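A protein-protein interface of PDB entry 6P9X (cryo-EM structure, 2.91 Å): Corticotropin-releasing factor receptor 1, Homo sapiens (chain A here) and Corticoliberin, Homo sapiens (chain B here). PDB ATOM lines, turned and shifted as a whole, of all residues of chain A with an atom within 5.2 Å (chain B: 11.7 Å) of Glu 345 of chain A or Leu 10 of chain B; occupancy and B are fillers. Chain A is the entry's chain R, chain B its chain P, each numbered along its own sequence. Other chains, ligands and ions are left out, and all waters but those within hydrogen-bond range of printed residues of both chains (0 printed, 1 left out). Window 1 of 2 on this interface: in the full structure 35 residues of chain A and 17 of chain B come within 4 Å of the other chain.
OH of Tyr 188 of chain A is in hydrogen-bond range of OG1 of Thr 11 of chain B (2.9 Å). OG of Ser 7 of chain B lies within hydrogen-bond range of O of Tyr 320 of chain A (2.8 Å). OE1 of Glu 345 of chain A lies close to O of Ser 7 of chain B, at 2.9 Å.
The guanidinium group of Arg 158 of chain A lies within hydrogen-bond range of the side-chain hydroxyl of Tyr 188 of chain A (2.9 Å). The side-chain amide oxygen (OE1) of Gln 348 of chain A sits at hydrogen-bond distance from the side-chain hydroxyl (OH) of Tyr 320 of chain A (3.0 Å).
Tyr 188 of chain A touches Phe 12 of chain B. Leu 8 of chain B touches His 192 of chain A. Tyr 320 of chain A touches Leu 8 of chain B (CD1 to CD2, 3.6 Å). Phe 337 of chain A touches Pro 5 of chain B. Leu 10 of chain B touches Ile 338 of chain A (CD1 to CD1, 3.8 Å). OD1 of Asn 341 of chain A touches CB of Ser 7 of chain B (3.2 Å). Asn 341 of chain A touches Leu 10 of chain B. Leu 10 of chain B touches Ser 342 of chain A (CD2 to OG, 3.5 Å). Glu 345 of chain A touches Leu 10 of chain B. OE2 of Glu 345 of chain A touches OG1 of Thr 11 of chain B, 3.5 Å away.
Printed residues of chain B within 4 Å of His 192 of chain A: Leu 8 (3.2 Å). Of the printed residues of chain B, Tyr 320 of chain A touches Ser 7 (2.8 Å) and Leu 8 (3.6 Å). Ile 338 of chain A touches three residues of chain B. Asn 341 of chain A touches just these residues of chain B: Ser 7 and Leu 10. Ser 342 of chain A touches just one residue of chain B: Leu 10. Of the printed residues of chain B, Glu 345 of chain A touches Ser 7, Leu 10 and Thr 11. No residue of chain B comes within 4 Å of Gln 348 of chain A. Printed residues of chain A within 4 Å of Ser 7 of chain B: Tyr 320 (2.8 Å), Asn 341 (3.2 Å) and Glu 345 (2.9 Å). Of the printed residues of chain A, Leu 10 of chain B touches Ile 338, Asn 341, Ser 342 and Glu 345.
Hydrophobic or aromatic side chains of chain A that line the printed part of chain B: Tyr 188, His 192, Tyr 320, Phe 337 and Ile 338. Hydrophobic or aromatic side chains of chain B within 4 Å of the printed part of chain A: Pro 5, Leu 8, Leu 10, Phe 12, His 13 and Leu 14.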
ATOM      1  N   HIS A 120      21.155 -20.872 -26.481  1.00  0.00           N
ATOM      2  CA  HIS A 120      21.830 -21.008 -27.765  1.00  0.00           C
ATOM      3  C   HIS A 120      22.837 -22.150 -27.786  1.00  0.00           C
ATOM      4  O   HIS A 120      23.384 -22.447 -28.852  1.00  0.00           O
ATOM      5  CB  HIS A 120      22.530 -19.698 -28.132  1.00  0.00           C
ATOM      6  CG  HIS A 120      21.596 -18.620 -28.587  1.00  0.00           C
ATOM      7  ND1 HIS A 120      21.223 -18.466 -29.904  1.00  0.00           N
ATOM      8  CD2 HIS A 120      20.964 -17.639 -27.900  1.00  0.00           C
ATOM      9  CE1 HIS A 120      20.400 -17.439 -30.008  1.00  0.00           C
ATOM     10  NE2 HIS A 120      20.227 -16.918 -28.807  1.00  0.00           N
ATOM     11  N   ARG A 158      22.575 -19.006 -37.671  1.00  0.00           N
ATOM     12  CA  ARG A 158      22.289 -17.858 -36.818  1.00  0.00           C
ATOM     13  C   ARG A 158      22.756 -18.100 -35.389  1.00  0.00           C
ATOM     14  O   ARG A 158      23.200 -17.169 -34.708  1.00  0.00           O
ATOM     15  CB  ARG A 158      20.797 -17.532 -36.848  1.00  0.00           C
ATOM     16  CG  ARG A 158      20.475 -16.153 -36.307  1.00  0.00           C
ATOM     17  CD  ARG A 158      19.041 -16.061 -35.828  1.00  0.00           C
ATOM     18  NE  ARG A 158      18.743 -17.047 -34.795  1.00  0.00           N
ATOM     19  CZ  ARG A 158      19.022 -16.888 -33.506  1.00  0.00           C
ATOM     20  NH1 ARG A 158      18.714 -17.841 -32.639  1.00  0.00           N
ATOM     21  NH2 ARG A 158      19.611 -15.779 -33.082  1.00  0.00           N
ATOM     22  N   TYR A 188      24.798 -11.314 -39.031  1.00  0.00           N
ATOM     23  CA  TYR A 188      23.788 -11.815 -38.106  1.00  0.00           C
ATOM     24  C   TYR A 188      22.392 -11.397 -38.550  1.00  0.00           C
ATOM     25  O   TYR A 188      21.427 -12.154 -38.398  1.00  0.00           O
ATOM     26  CB  TYR A 188      24.071 -11.320 -36.688  1.00  0.00           C
ATOM     27  CG  TYR A 188      23.022 -11.752 -35.688  1.00  0.00           C
ATOM     28  CD1 TYR A 188      23.087 -12.997 -35.083  1.00  0.00           C
ATOM     29  CD2 TYR A 188      21.962 -10.920 -35.358  1.00  0.00           C
ATOM     30  CE1 TYR A 188      22.130 -13.399 -34.177  1.00  0.00           C
ATOM     31  CE2 TYR A 188      20.999 -11.314 -34.456  1.00  0.00           C
ATOM     32  CZ  TYR A 188      21.088 -12.554 -33.868  1.00  0.00           C
ATOM     33  OH  TYR A 188      20.134 -12.954 -32.963  1.00  0.00           O
ATOM     34  N   HIS A 192      19.318 -13.885 -39.512  1.00  0.00           N
ATOM     35  CA  HIS A 192      18.095 -13.735 -38.734  1.00  0.00           C
ATOM     36  C   HIS A 192      16.888 -13.547 -39.643  1.00  0.00           C
ATOM     37  O   HIS A 192      15.779 -13.979 -39.313  1.00  0.00           O
ATOM     38  CB  HIS A 192      18.228 -12.561 -37.767  1.00  0.00           C
ATOM     39  CG  HIS A 192      17.207 -12.559 -36.674  1.00  0.00           C
ATOM     40  ND1 HIS A 192      16.634 -11.402 -36.192  1.00  0.00           N
ATOM     41  CD2 HIS A 192      16.654 -13.574 -35.968  1.00  0.00           C
ATOM     42  CE1 HIS A 192      15.773 -11.705 -35.238  1.00  0.00           C
ATOM     43  NE2 HIS A 192      15.767 -13.016 -35.083  1.00  0.00           N
ATOM     44  N   TYR A 320       7.501 -14.874 -31.436  1.00  0.00           N
ATOM     45  CA  TYR A 320       7.856 -13.463 -31.455  1.00  0.00           C
ATOM     46  C   TYR A 320       6.646 -12.558 -31.283  1.00  0.00           C
ATOM     47  O   TYR A 320       6.816 -11.361 -31.032  1.00  0.00           O
ATOM     48  CB  TYR A 320       8.568 -13.112 -32.761  1.00  0.00           C
ATOM     49  CG  TYR A 320       9.889 -13.815 -32.961  1.00  0.00           C
ATOM     50  CD1 TYR A 320      11.071 -13.252 -32.506  1.00  0.00           C
ATOM     51  CD2 TYR A 320       9.954 -15.036 -33.613  1.00  0.00           C
ATOM     52  CE1 TYR A 320      12.280 -13.888 -32.688  1.00  0.00           C
ATOM     53  CE2 TYR A 320      11.157 -15.680 -33.799  1.00  0.00           C
ATOM     54  CZ  TYR A 320      12.317 -15.102 -33.336  1.00  0.00           C
ATOM     55  OH  TYR A 320      13.520 -15.742 -33.521  1.00  0.00           O
ATOM     56  N   PHE A 337       9.400  -8.998 -20.147  1.00  0.00           N
ATOM     57  CA  PHE A 337       9.659  -8.918 -21.582  1.00  0.00           C
ATOM     58  C   PHE A 337      11.029  -9.481 -21.932  1.00  0.00           C
ATOM     59  O   PHE A 337      11.182 -10.186 -22.935  1.00  0.00           O
ATOM     60  CB  PHE A 337       9.540  -7.469 -22.055  1.00  0.00           C
ATOM     61  CG  PHE A 337      10.048  -7.238 -23.452  1.00  0.00           C
ATOM     62  CD1 PHE A 337       9.240  -7.480 -24.545  1.00  0.00           C
ATOM     63  CD2 PHE A 337      11.330  -6.767 -23.669  1.00  0.00           C
ATOM     64  CE1 PHE A 337       9.701  -7.269 -25.826  1.00  0.00           C
ATOM     65  CE2 PHE A 337      11.797  -6.556 -24.948  1.00  0.00           C
ATOM     66  CZ  PHE A 337      10.979  -6.806 -26.027  1.00  0.00           C
ATOM     67  N   ILE A 338      12.039  -9.182 -21.115  1.00  0.00           N
ATOM     68  CA  ILE A 338      13.383  -9.680 -21.389  1.00  0.00           C
ATOM     69  C   ILE A 338      13.465 -11.177 -21.117  1.00  0.00           C
ATOM     70  O   ILE A 338      14.077 -11.929 -21.884  1.00  0.00           O
ATOM     71  CB  ILE A 338      14.422  -8.893 -20.571  1.00  0.00           C
ATOM     72  CG1 ILE A 338      14.353  -7.406 -20.909  1.00  0.00           C
ATOM     73  CG2 ILE A 338      15.811  -9.402 -20.852  1.00  0.00           C
ATOM     74  CD1 ILE A 338      14.615  -7.099 -22.361  1.00  0.00           C
ATOM     75  N   ASN A 341      11.135 -13.294 -23.685  1.00  0.00           N
ATOM     76  CA  ASN A 341      11.637 -13.298 -25.050  1.00  0.00           C
ATOM     77  C   ASN A 341      13.026 -13.901 -25.179  1.00  0.00           C
ATOM     78  O   ASN A 341      13.410 -14.292 -26.286  1.00  0.00           O
ATOM     79  CB  ASN A 341      11.654 -11.875 -25.616  1.00  0.00           C
ATOM     80  CG  ASN A 341      10.267 -11.309 -25.792  1.00  0.00           C
ATOM     81  OD1 ASN A 341       9.619 -11.535 -26.810  1.00  0.00           O
ATOM     82  ND2 ASN A 341       9.800 -10.571 -24.798  1.00  0.00           N
ATOM     83  N   SER A 342      13.789 -13.982 -24.089  1.00  0.00           N
ATOM     84  CA  SER A 342      15.077 -14.664 -24.139  1.00  0.00           C
ATOM     85  C   SER A 342      14.915 -16.175 -24.073  1.00  0.00           C
ATOM     86  O   SER A 342      15.806 -16.910 -24.512  1.00  0.00           O
ATOM     87  CB  SER A 342      15.975 -14.186 -23.000  1.00  0.00           C
ATOM     88  OG  SER A 342      15.948 -12.776 -22.885  1.00  0.00           O
ATOM     89  N   PHE A 343      13.797 -16.653 -23.531  1.00  0.00           N
ATOM     90  CA  PHE A 343      13.561 -18.090 -23.466  1.00  0.00           C
ATOM     91  C   PHE A 343      12.973 -18.606 -24.772  1.00  0.00           C
ATOM     92  O   PHE A 343      13.263 -19.730 -25.193  1.00  0.00           O
ATOM     93  CB  PHE A 343      12.638 -18.414 -22.292  1.00  0.00           C
ATOM     94  CG  PHE A 343      12.236 -19.856 -22.222  1.00  0.00           C
ATOM     95  CD1 PHE A 343      13.137 -20.820 -21.813  1.00  0.00           C
ATOM     96  CD2 PHE A 343      10.955 -20.249 -22.571  1.00  0.00           C
ATOM     97  CE1 PHE A 343      12.772 -22.147 -21.751  1.00  0.00           C
ATOM     98  CE2 PHE A 343      10.583 -21.575 -22.511  1.00  0.00           C
ATOM     99  CZ  PHE A 343      11.492 -22.525 -22.100  1.00  0.00           C
ATOM    100  N   LEU A 344      12.141 -17.797 -25.429  1.00  0.00           N
ATOM    101  CA  LEU A 344      11.515 -18.235 -26.671  1.00  0.00           C
ATOM    102  C   LEU A 344      12.473 -18.100 -27.847  1.00  0.00           C
ATOM    103  O   LEU A 344      12.501 -18.953 -28.740  1.00  0.00           O
ATOM    104  CB  LEU A 344      10.237 -17.436 -26.921  1.00  0.00           C
ATOM    105  CG  LEU A 344       9.096 -17.665 -25.931  1.00  0.00           C
ATOM    106  CD1 LEU A 344       7.868 -16.878 -26.344  1.00  0.00           C
ATOM    107  CD2 LEU A 344       8.774 -19.143 -25.822  1.00  0.00           C
ATOM    108  N   GLU A 345      13.267 -17.029 -27.865  1.00  0.00           N
ATOM    109  CA  GLU A 345      14.168 -16.793 -28.989  1.00  0.00           C
ATOM    110  C   GLU A 345      15.330 -17.777 -28.982  1.00  0.00           C
ATOM    111  O   GLU A 345      15.697 -18.332 -30.025  1.00  0.00           O
ATOM    112  CB  GLU A 345      14.685 -15.356 -28.950  1.00  0.00           C
ATOM    113  CG  GLU A 345      15.423 -14.919 -30.202  1.00  0.00           C
ATOM    114  CD  GLU A 345      15.282 -13.433 -30.470  1.00  0.00           C
ATOM    115  OE1 GLU A 345      14.230 -12.863 -30.115  1.00  0.00           O
ATOM    116  OE2 GLU A 345      16.224 -12.836 -31.031  1.00  0.00           O
ATOM    117  N   SER A 346      15.927 -18.004 -27.812  1.00  0.00           N
ATOM    118  CA  SER A 346      17.113 -18.851 -27.743  1.00  0.00           C
ATOM    119  C   SER A 346      16.756 -20.326 -27.873  1.00  0.00           C
ATOM    120  O   SER A 346      17.477 -21.091 -28.523  1.00  0.00           O
ATOM    121  CB  SER A 346      17.864 -18.592 -26.439  1.00  0.00           C
ATOM    122  OG  SER A 346      16.984 -18.625 -25.331  1.00  0.00           O
ATOM    123  N   PHE A 347      15.650 -20.746 -27.265  1.00  0.00           N
ATOM    124  CA  PHE A 347      15.233 -22.140 -27.296  1.00  0.00           C
ATOM    125  C   PHE A 347      14.357 -22.479 -28.494  1.00  0.00           C
ATOM    126  O   PHE A 347      13.686 -23.515 -28.474  1.00  0.00           O
ATOM    127  CB  PHE A 347      14.482 -22.498 -26.010  1.00  0.00           C
ATOM    128  CG  PHE A 347      15.375 -22.725 -24.827  1.00  0.00           C
ATOM    129  CD1 PHE A 347      15.723 -21.676 -23.996  1.00  0.00           C
ATOM    130  CD2 PHE A 347      15.858 -23.989 -24.541  1.00  0.00           C
ATOM    131  CE1 PHE A 347      16.539 -21.881 -22.903  1.00  0.00           C
ATOM    132  CE2 PHE A 347      16.675 -24.199 -23.451  1.00  0.00           C
ATOM    133  CZ  PHE A 347      17.017 -23.143 -22.632  1.00  0.00           C
ATOM    134  N   GLN A 348      14.340 -21.642 -29.532  1.00  0.00           N
ATOM    135  CA  GLN A 348      13.492 -21.933 -30.683  1.00  0.00           C
ATOM    136  C   GLN A 348      14.083 -23.044 -31.538  1.00  0.00           C
ATOM    137  O   GLN A 348      13.357 -23.926 -32.010  1.00  0.00           O
ATOM    138  CB  GLN A 348      13.281 -20.675 -31.520  1.00  0.00           C
ATOM    139  CG  GLN A 348      12.302 -20.877 -32.658  1.00  0.00           C
ATOM    140  CD  GLN A 348      12.077 -19.623 -33.463  1.00  0.00           C
ATOM    141  OE1 GLN A 348      12.776 -18.626 -33.285  1.00  0.00           O
ATOM    142  NE2 GLN A 348      11.099 -19.662 -34.356  1.00  0.00           N
ATOM    143  N   GLY A 349      15.398 -23.015 -31.758  1.00  0.00           N
ATOM    144  CA  GLY A 349      16.029 -24.077 -32.524  1.00  0.00           C
ATOM    145  C   GLY A 349      15.932 -25.421 -31.833  1.00  0.00           C
ATOM    146  O   GLY A 349      15.931 -26.468 -32.484  1.00  0.00           O
ATOM    147  N   GLU B   3      12.585   4.564 -27.027  1.00  0.00           N
ATOM    148  CA  GLU B   3      11.880   3.626 -27.889  1.00  0.00           C
ATOM    149  C   GLU B   3      11.755   2.272 -27.196  1.00  0.00           C
ATOM    150  O   GLU B   3      12.743   1.772 -26.641  1.00  0.00           O
ATOM    151  CB  GLU B   3      12.612   3.472 -29.220  1.00  0.00           C
ATOM    152  CG  GLU B   3      12.629   4.731 -30.070  1.00  0.00           C
ATOM    153  CD  GLU B   3      11.256   5.110 -30.583  1.00  0.00           C
ATOM    154  OE1 GLU B   3      10.439   4.197 -30.826  1.00  0.00           O
ATOM    155  OE2 GLU B   3      10.992   6.320 -30.743  1.00  0.00           O
ATOM    156  N   PRO B   4      10.577   1.656 -27.199  1.00  0.00           N
ATOM    157  CA  PRO B   4      10.418   0.357 -26.545  1.00  0.00           C
ATOM    158  C   PRO B   4      11.033  -0.750 -27.380  1.00  0.00           C
ATOM    159  O   PRO B   4      10.974  -0.712 -28.619  1.00  0.00           O
ATOM    160  CB  PRO B   4       8.894   0.200 -26.445  1.00  0.00           C
ATOM    161  CG  PRO B   4       8.372   0.980 -27.601  1.00  0.00           C
ATOM    162  CD  PRO B   4       9.323   2.133 -27.806  1.00  0.00           C
ATOM    163  N   PRO B   5      11.637  -1.749 -26.743  1.00  0.00           N
ATOM    164  CA  PRO B   5      12.219  -2.858 -27.505  1.00  0.00           C
ATOM    165  C   PRO B   5      11.140  -3.796 -28.022  1.00  0.00           C
ATOM    166  O   PRO B   5      10.132  -4.037 -27.357  1.00  0.00           O
ATOM    167  CB  PRO B   5      13.127  -3.557 -26.484  1.00  0.00           C
ATOM    168  CG  PRO B   5      13.100  -2.700 -25.244  1.00  0.00           C
ATOM    169  CD  PRO B   5      11.845  -1.908 -25.298  1.00  0.00           C
ATOM    170  N   ILE B   6      11.361  -4.325 -29.218  1.00  0.00           N
ATOM    171  CA  ILE B   6      10.495  -5.337 -29.782  1.00  0.00           C
ATOM    172  C   ILE B   6      11.192  -6.688 -29.682  1.00  0.00           C
ATOM    173  O   ILE B   6      12.382  -6.778 -29.393  1.00  0.00           O
ATOM    174  CB  ILE B   6      10.094  -5.008 -31.238  1.00  0.00           C
ATOM    175  CG1 ILE B   6      11.315  -5.037 -32.154  1.00  0.00           C
ATOM    176  CG2 ILE B   6       9.413  -3.656 -31.306  1.00  0.00           C
ATOM    177  CD1 ILE B   6      11.005  -4.653 -33.579  1.00  0.00           C
ATOM    178  N   SER B   7      10.436  -7.761 -29.917  1.00  0.00           N
ATOM    179  CA  SER B   7      10.978  -9.100 -29.709  1.00  0.00           C
ATOM    180  C   SER B   7      11.976  -9.476 -30.797  1.00  0.00           C
ATOM    181  O   SER B   7      12.842 -10.331 -30.580  1.00  0.00           O
ATOM    182  CB  SER B   7       9.840 -10.117 -29.646  1.00  0.00           C
ATOM    183  OG  SER B   7       9.443 -10.516 -30.943  1.00  0.00           O
ATOM    184  N   LEU B   8      11.873  -8.854 -31.972  1.00  0.00           N
ATOM    185  CA  LEU B   8      12.800  -9.144 -33.060  1.00  0.00           C
ATOM    186  C   LEU B   8      14.198  -8.600 -32.807  1.00  0.00           C
ATOM    187  O   LEU B   8      15.162  -9.152 -33.343  1.00  0.00           O
ATOM    188  CB  LEU B   8      12.272  -8.572 -34.376  1.00  0.00           C
ATOM    189  CG  LEU B   8      10.842  -8.911 -34.786  1.00  0.00           C
ATOM    190  CD1 LEU B   8      10.593  -8.459 -36.210  1.00  0.00           C
ATOM    191  CD2 LEU B   8      10.580 -10.395 -34.644  1.00  0.00           C
ATOM    192  N   ASP B   9      14.329  -7.537 -32.014  1.00  0.00           N
ATOM    193  CA  ASP B   9      15.608  -6.887 -31.768  1.00  0.00           C
ATOM    194  C   ASP B   9      16.087  -7.119 -30.339  1.00  0.00           C
ATOM    195  O   ASP B   9      16.583  -6.195 -29.691  1.00  0.00           O
ATOM    196  CB  ASP B   9      15.494  -5.392 -32.083  1.00  0.00           C
ATOM    197  CG  ASP B   9      16.844  -4.699 -32.198  1.00  0.00           C
ATOM    198  OD1 ASP B   9      17.372  -4.213 -31.177  1.00  0.00           O
ATOM    199  OD2 ASP B   9      17.362  -4.603 -33.330  1.00  0.00           O
ATOM    200  N   LEU B  10      15.922  -8.337 -29.821  1.00  0.00           N
ATOM    201  CA  LEU B  10      16.285  -8.598 -28.434  1.00  0.00           C
ATOM    202  C   LEU B  10      17.784  -8.823 -28.282  1.00  0.00           C
ATOM    203  O   LEU B  10      18.375  -8.442 -27.266  1.00  0.00           O
ATOM    204  CB  LEU B  10      15.516  -9.807 -27.907  1.00  0.00           C
ATOM    205  CG  LEU B  10      15.699 -10.058 -26.412  1.00  0.00           C
ATOM    206  CD1 LEU B  10      14.965  -8.998 -25.611  1.00  0.00           C
ATOM    207  CD2 LEU B  10      15.247 -11.447 -26.033  1.00  0.00           C
ATOM    208  N   THR B  11      18.414  -9.449 -29.276  1.00  0.00           N
ATOM    209  CA  THR B  11      19.832  -9.771 -29.176  1.00  0.00           C
ATOM    210  C   THR B  11      20.680  -8.507 -29.097  1.00  0.00           C
ATOM    211  O   THR B  11      21.578  -8.393 -28.259  1.00  0.00           O
ATOM    212  CB  THR B  11      20.259 -10.634 -30.363  1.00  0.00           C
ATOM    213  OG1 THR B  11      19.543 -11.875 -30.331  1.00  0.00           O
ATOM    214  CG2 THR B  11      21.749 -10.916 -30.309  1.00  0.00           C
ATOM    215  N   PHE B  12      20.400  -7.541 -29.972  1.00  0.00           N
ATOM    216  CA  PHE B  12      21.172  -6.304 -29.958  1.00  0.00           C
ATOM    217  C   PHE B  12      20.673  -5.343 -28.891  1.00  0.00           C
ATOM    218  O   PHE B  12      21.344  -4.351 -28.594  1.00  0.00           O
ATOM    219  CB  PHE B  12      21.137  -5.647 -31.334  1.00  0.00           C
ATOM    220  CG  PHE B  12      21.927  -6.388 -32.369  1.00  0.00           C
ATOM    221  CD1 PHE B  12      23.201  -6.842 -32.087  1.00  0.00           C
ATOM    222  CD2 PHE B  12      21.396  -6.636 -33.619  1.00  0.00           C
ATOM    223  CE1 PHE B  12      23.931  -7.528 -33.030  1.00  0.00           C
ATOM    224  CE2 PHE B  12      22.125  -7.322 -34.566  1.00  0.00           C
ATOM    225  CZ  PHE B  12      23.392  -7.768 -34.271  1.00  0.00           C
ATOM    226  N   HIS B  13      19.502  -5.609 -28.310  1.00  0.00           N
ATOM    227  CA  HIS B  13      19.059  -4.824 -27.163  1.00  0.00           C
ATOM    228  C   HIS B  13      19.816  -5.234 -25.908  1.00  0.00           C
ATOM    229  O   HIS B  13      20.287  -4.384 -25.147  1.00  0.00           O
ATOM    230  CB  HIS B  13      17.553  -4.979 -26.961  1.00  0.00           C
ATOM    231  CG  HIS B  13      17.043  -4.329 -25.713  1.00  0.00           C
ATOM    232  ND1 HIS B  13      16.457  -5.041 -24.690  1.00  0.00           N
ATOM    233  CD2 HIS B  13      17.037  -3.034 -25.322  1.00  0.00           C
ATOM    234  CE1 HIS B  13      16.112  -4.213 -23.722  1.00  0.00           C
ATOM    235  NE2 HIS B  13      16.452  -2.988 -24.080  1.00  0.00           N
ATOM    236  N   LEU B  14      19.943  -6.543 -25.678  1.00  0.00           N
ATOM    237  CA  LEU B  14      20.755  -7.021 -24.565  1.00  0.00           C
ATOM    238  C   LEU B  14      22.215  -6.633 -24.748  1.00  0.00           C
ATOM    239  O   LEU B  14      22.928  -6.389 -23.768  1.00  0.00           O
ATOM    240  CB  LEU B  14      20.621  -8.536 -24.428  1.00  0.00           C
ATOM    241  CG  LEU B  14      19.313  -9.070 -23.849  1.00  0.00           C
ATOM    242  CD1 LEU B  14      19.440 -10.551 -23.555  1.00  0.00           C
ATOM    243  CD2 LEU B  14      18.932  -8.305 -22.595  1.00  0.00           C
ATOM    244  N   LEU B  15      22.680  -6.578 -25.997  1.00  0.00           N
ATOM    245  CA  LEU B  15      24.049  -6.152 -26.254  1.00  0.00           C
ATOM    246  C   LEU B  15      24.214  -4.661 -25.999  1.00  0.00           C
ATOM    247  O   LEU B  15      25.219  -4.231 -25.425  1.00  0.00           O
ATOM    248  CB  LEU B  15      24.446  -6.501 -27.687  1.00  0.00           C
ATOM    249  CG  LEU B  15      25.911  -6.860 -27.923  1.00  0.00           C
ATOM    250  CD1 LEU B  15      26.269  -8.136 -27.186  1.00  0.00           C
ATOM    251  CD2 LEU B  15      26.194  -7.002 -29.405  1.00  0.00           C
ATOM    252  N   ARG B  16      23.234  -3.856 -26.410  1.00  0.00           N
ATOM    253  CA  ARG B  16      23.322  -2.417 -26.184  1.00  0.00           C
ATOM    254  C   ARG B  16      23.199  -2.082 -24.704  1.00  0.00           C
ATOM    255  O   ARG B  16      23.699  -1.046 -24.251  1.00  0.00           O
ATOM    256  CB  ARG B  16      22.241  -1.693 -26.985  1.00  0.00           C
ATOM    257  CG  ARG B  16      22.627  -1.377 -28.415  1.00  0.00           C
ATOM    258  CD  ARG B  16      21.643  -0.406 -29.041  1.00  0.00           C
ATOM    259  NE  ARG B  16      20.266  -0.880 -28.946  1.00  0.00           N
ATOM    260  CZ  ARG B  16      19.644  -1.570 -29.896  1.00  0.00           C
ATOM    261  NH1 ARG B  16      20.275  -1.871 -31.023  1.00  0.00           N
ATOM    262  NH2 ARG B  16      18.391  -1.959 -29.722  1.00  0.00           N
ATOM    263  N   GLU B  17      22.533  -2.944 -23.935  1.00  0.00           N
ATOM    264  CA  GLU B  17      22.362  -2.679 -22.510  1.00  0.00           C
ATOM    265  C   GLU B  17      23.645  -2.955 -21.740  1.00  0.00           C
ATOM    266  O   GLU B  17      23.998  -2.204 -20.823  1.00  0.00           O
ATOM    267  CB  GLU B  17      21.213  -3.515 -21.951  1.00  0.00           C
ATOM    268  CG  GLU B  17      19.829  -2.988 -22.294  1.00  0.00           C
ATOM    269  CD  GLU B  17      19.787  -1.479 -22.410  1.00  0.00           C
ATOM    270  OE1 GLU B  17      19.794  -0.800 -21.363  1.00  0.00           O
ATOM    271  OE2 GLU B  17      19.741  -0.971 -23.550  1.00  0.00           O
ATOM    272  N   VAL B  18      24.356  -4.027 -22.091  1.00  0.00           N
ATOM    273  CA  VAL B  18      25.583  -4.370 -21.376  1.00  0.00           C
ATOM    274  C   VAL B  18      26.739  -3.494 -21.847  1.00  0.00           C
ATOM    275  O   VAL B  18      27.684  -3.230 -21.099  1.00  0.00           O
ATOM    276  CB  VAL B  18      25.906  -5.866 -21.537  1.00  0.00           C
ATOM    277  CG1 VAL B  18      24.797  -6.715 -20.944  1.00  0.00           C
ATOM    278  CG2 VAL B  18      26.124  -6.215 -22.995  1.00  0.00           C
ATOM    279  N   LEU B  19      26.676  -3.021 -23.092  1.00  0.00           N
ATOM    280  CA  LEU B  19      27.758  -2.209 -23.635  1.00  0.00           C
ATOM    281  C   LEU B  19      27.729  -0.802 -23.052  1.00  0.00           C
ATOM    282  O   LEU B  19      28.716  -0.066 -23.146  1.00  0.00           O
ATOM    283  CB  LEU B  19      27.686  -2.160 -25.161  1.00  0.00           C
ATOM    284  CG  LEU B  19      28.238  -3.390 -25.881  1.00  0.00           C
ATOM    285  CD1 LEU B  19      28.391  -3.122 -27.365  1.00  0.00           C
ATOM    286  CD2 LEU B  19      29.559  -3.819 -25.273  1.00  0.00           C
ATOM    287  N   MET B  21      26.375  -0.722 -19.761  1.00  0.00           N
ATOM    288  CA  MET B  21      26.475  -1.111 -18.363  1.00  0.00           C
ATOM    289  C   MET B  21      27.874  -1.572 -17.981  1.00  0.00           C
ATOM    290  O   MET B  21      28.363  -1.192 -16.911  1.00  0.00           O
ATOM    291  CB  MET B  21      25.463  -2.220 -18.053  1.00  0.00           C
ATOM    292  CG  MET B  21      25.631  -2.883 -16.705  1.00  0.00           C
ATOM    293  SD  MET B  21      24.208  -3.913 -16.307  1.00  0.00           S
ATOM    294  CE  MET B  21      24.092  -4.911 -17.788  1.00  0.00           C
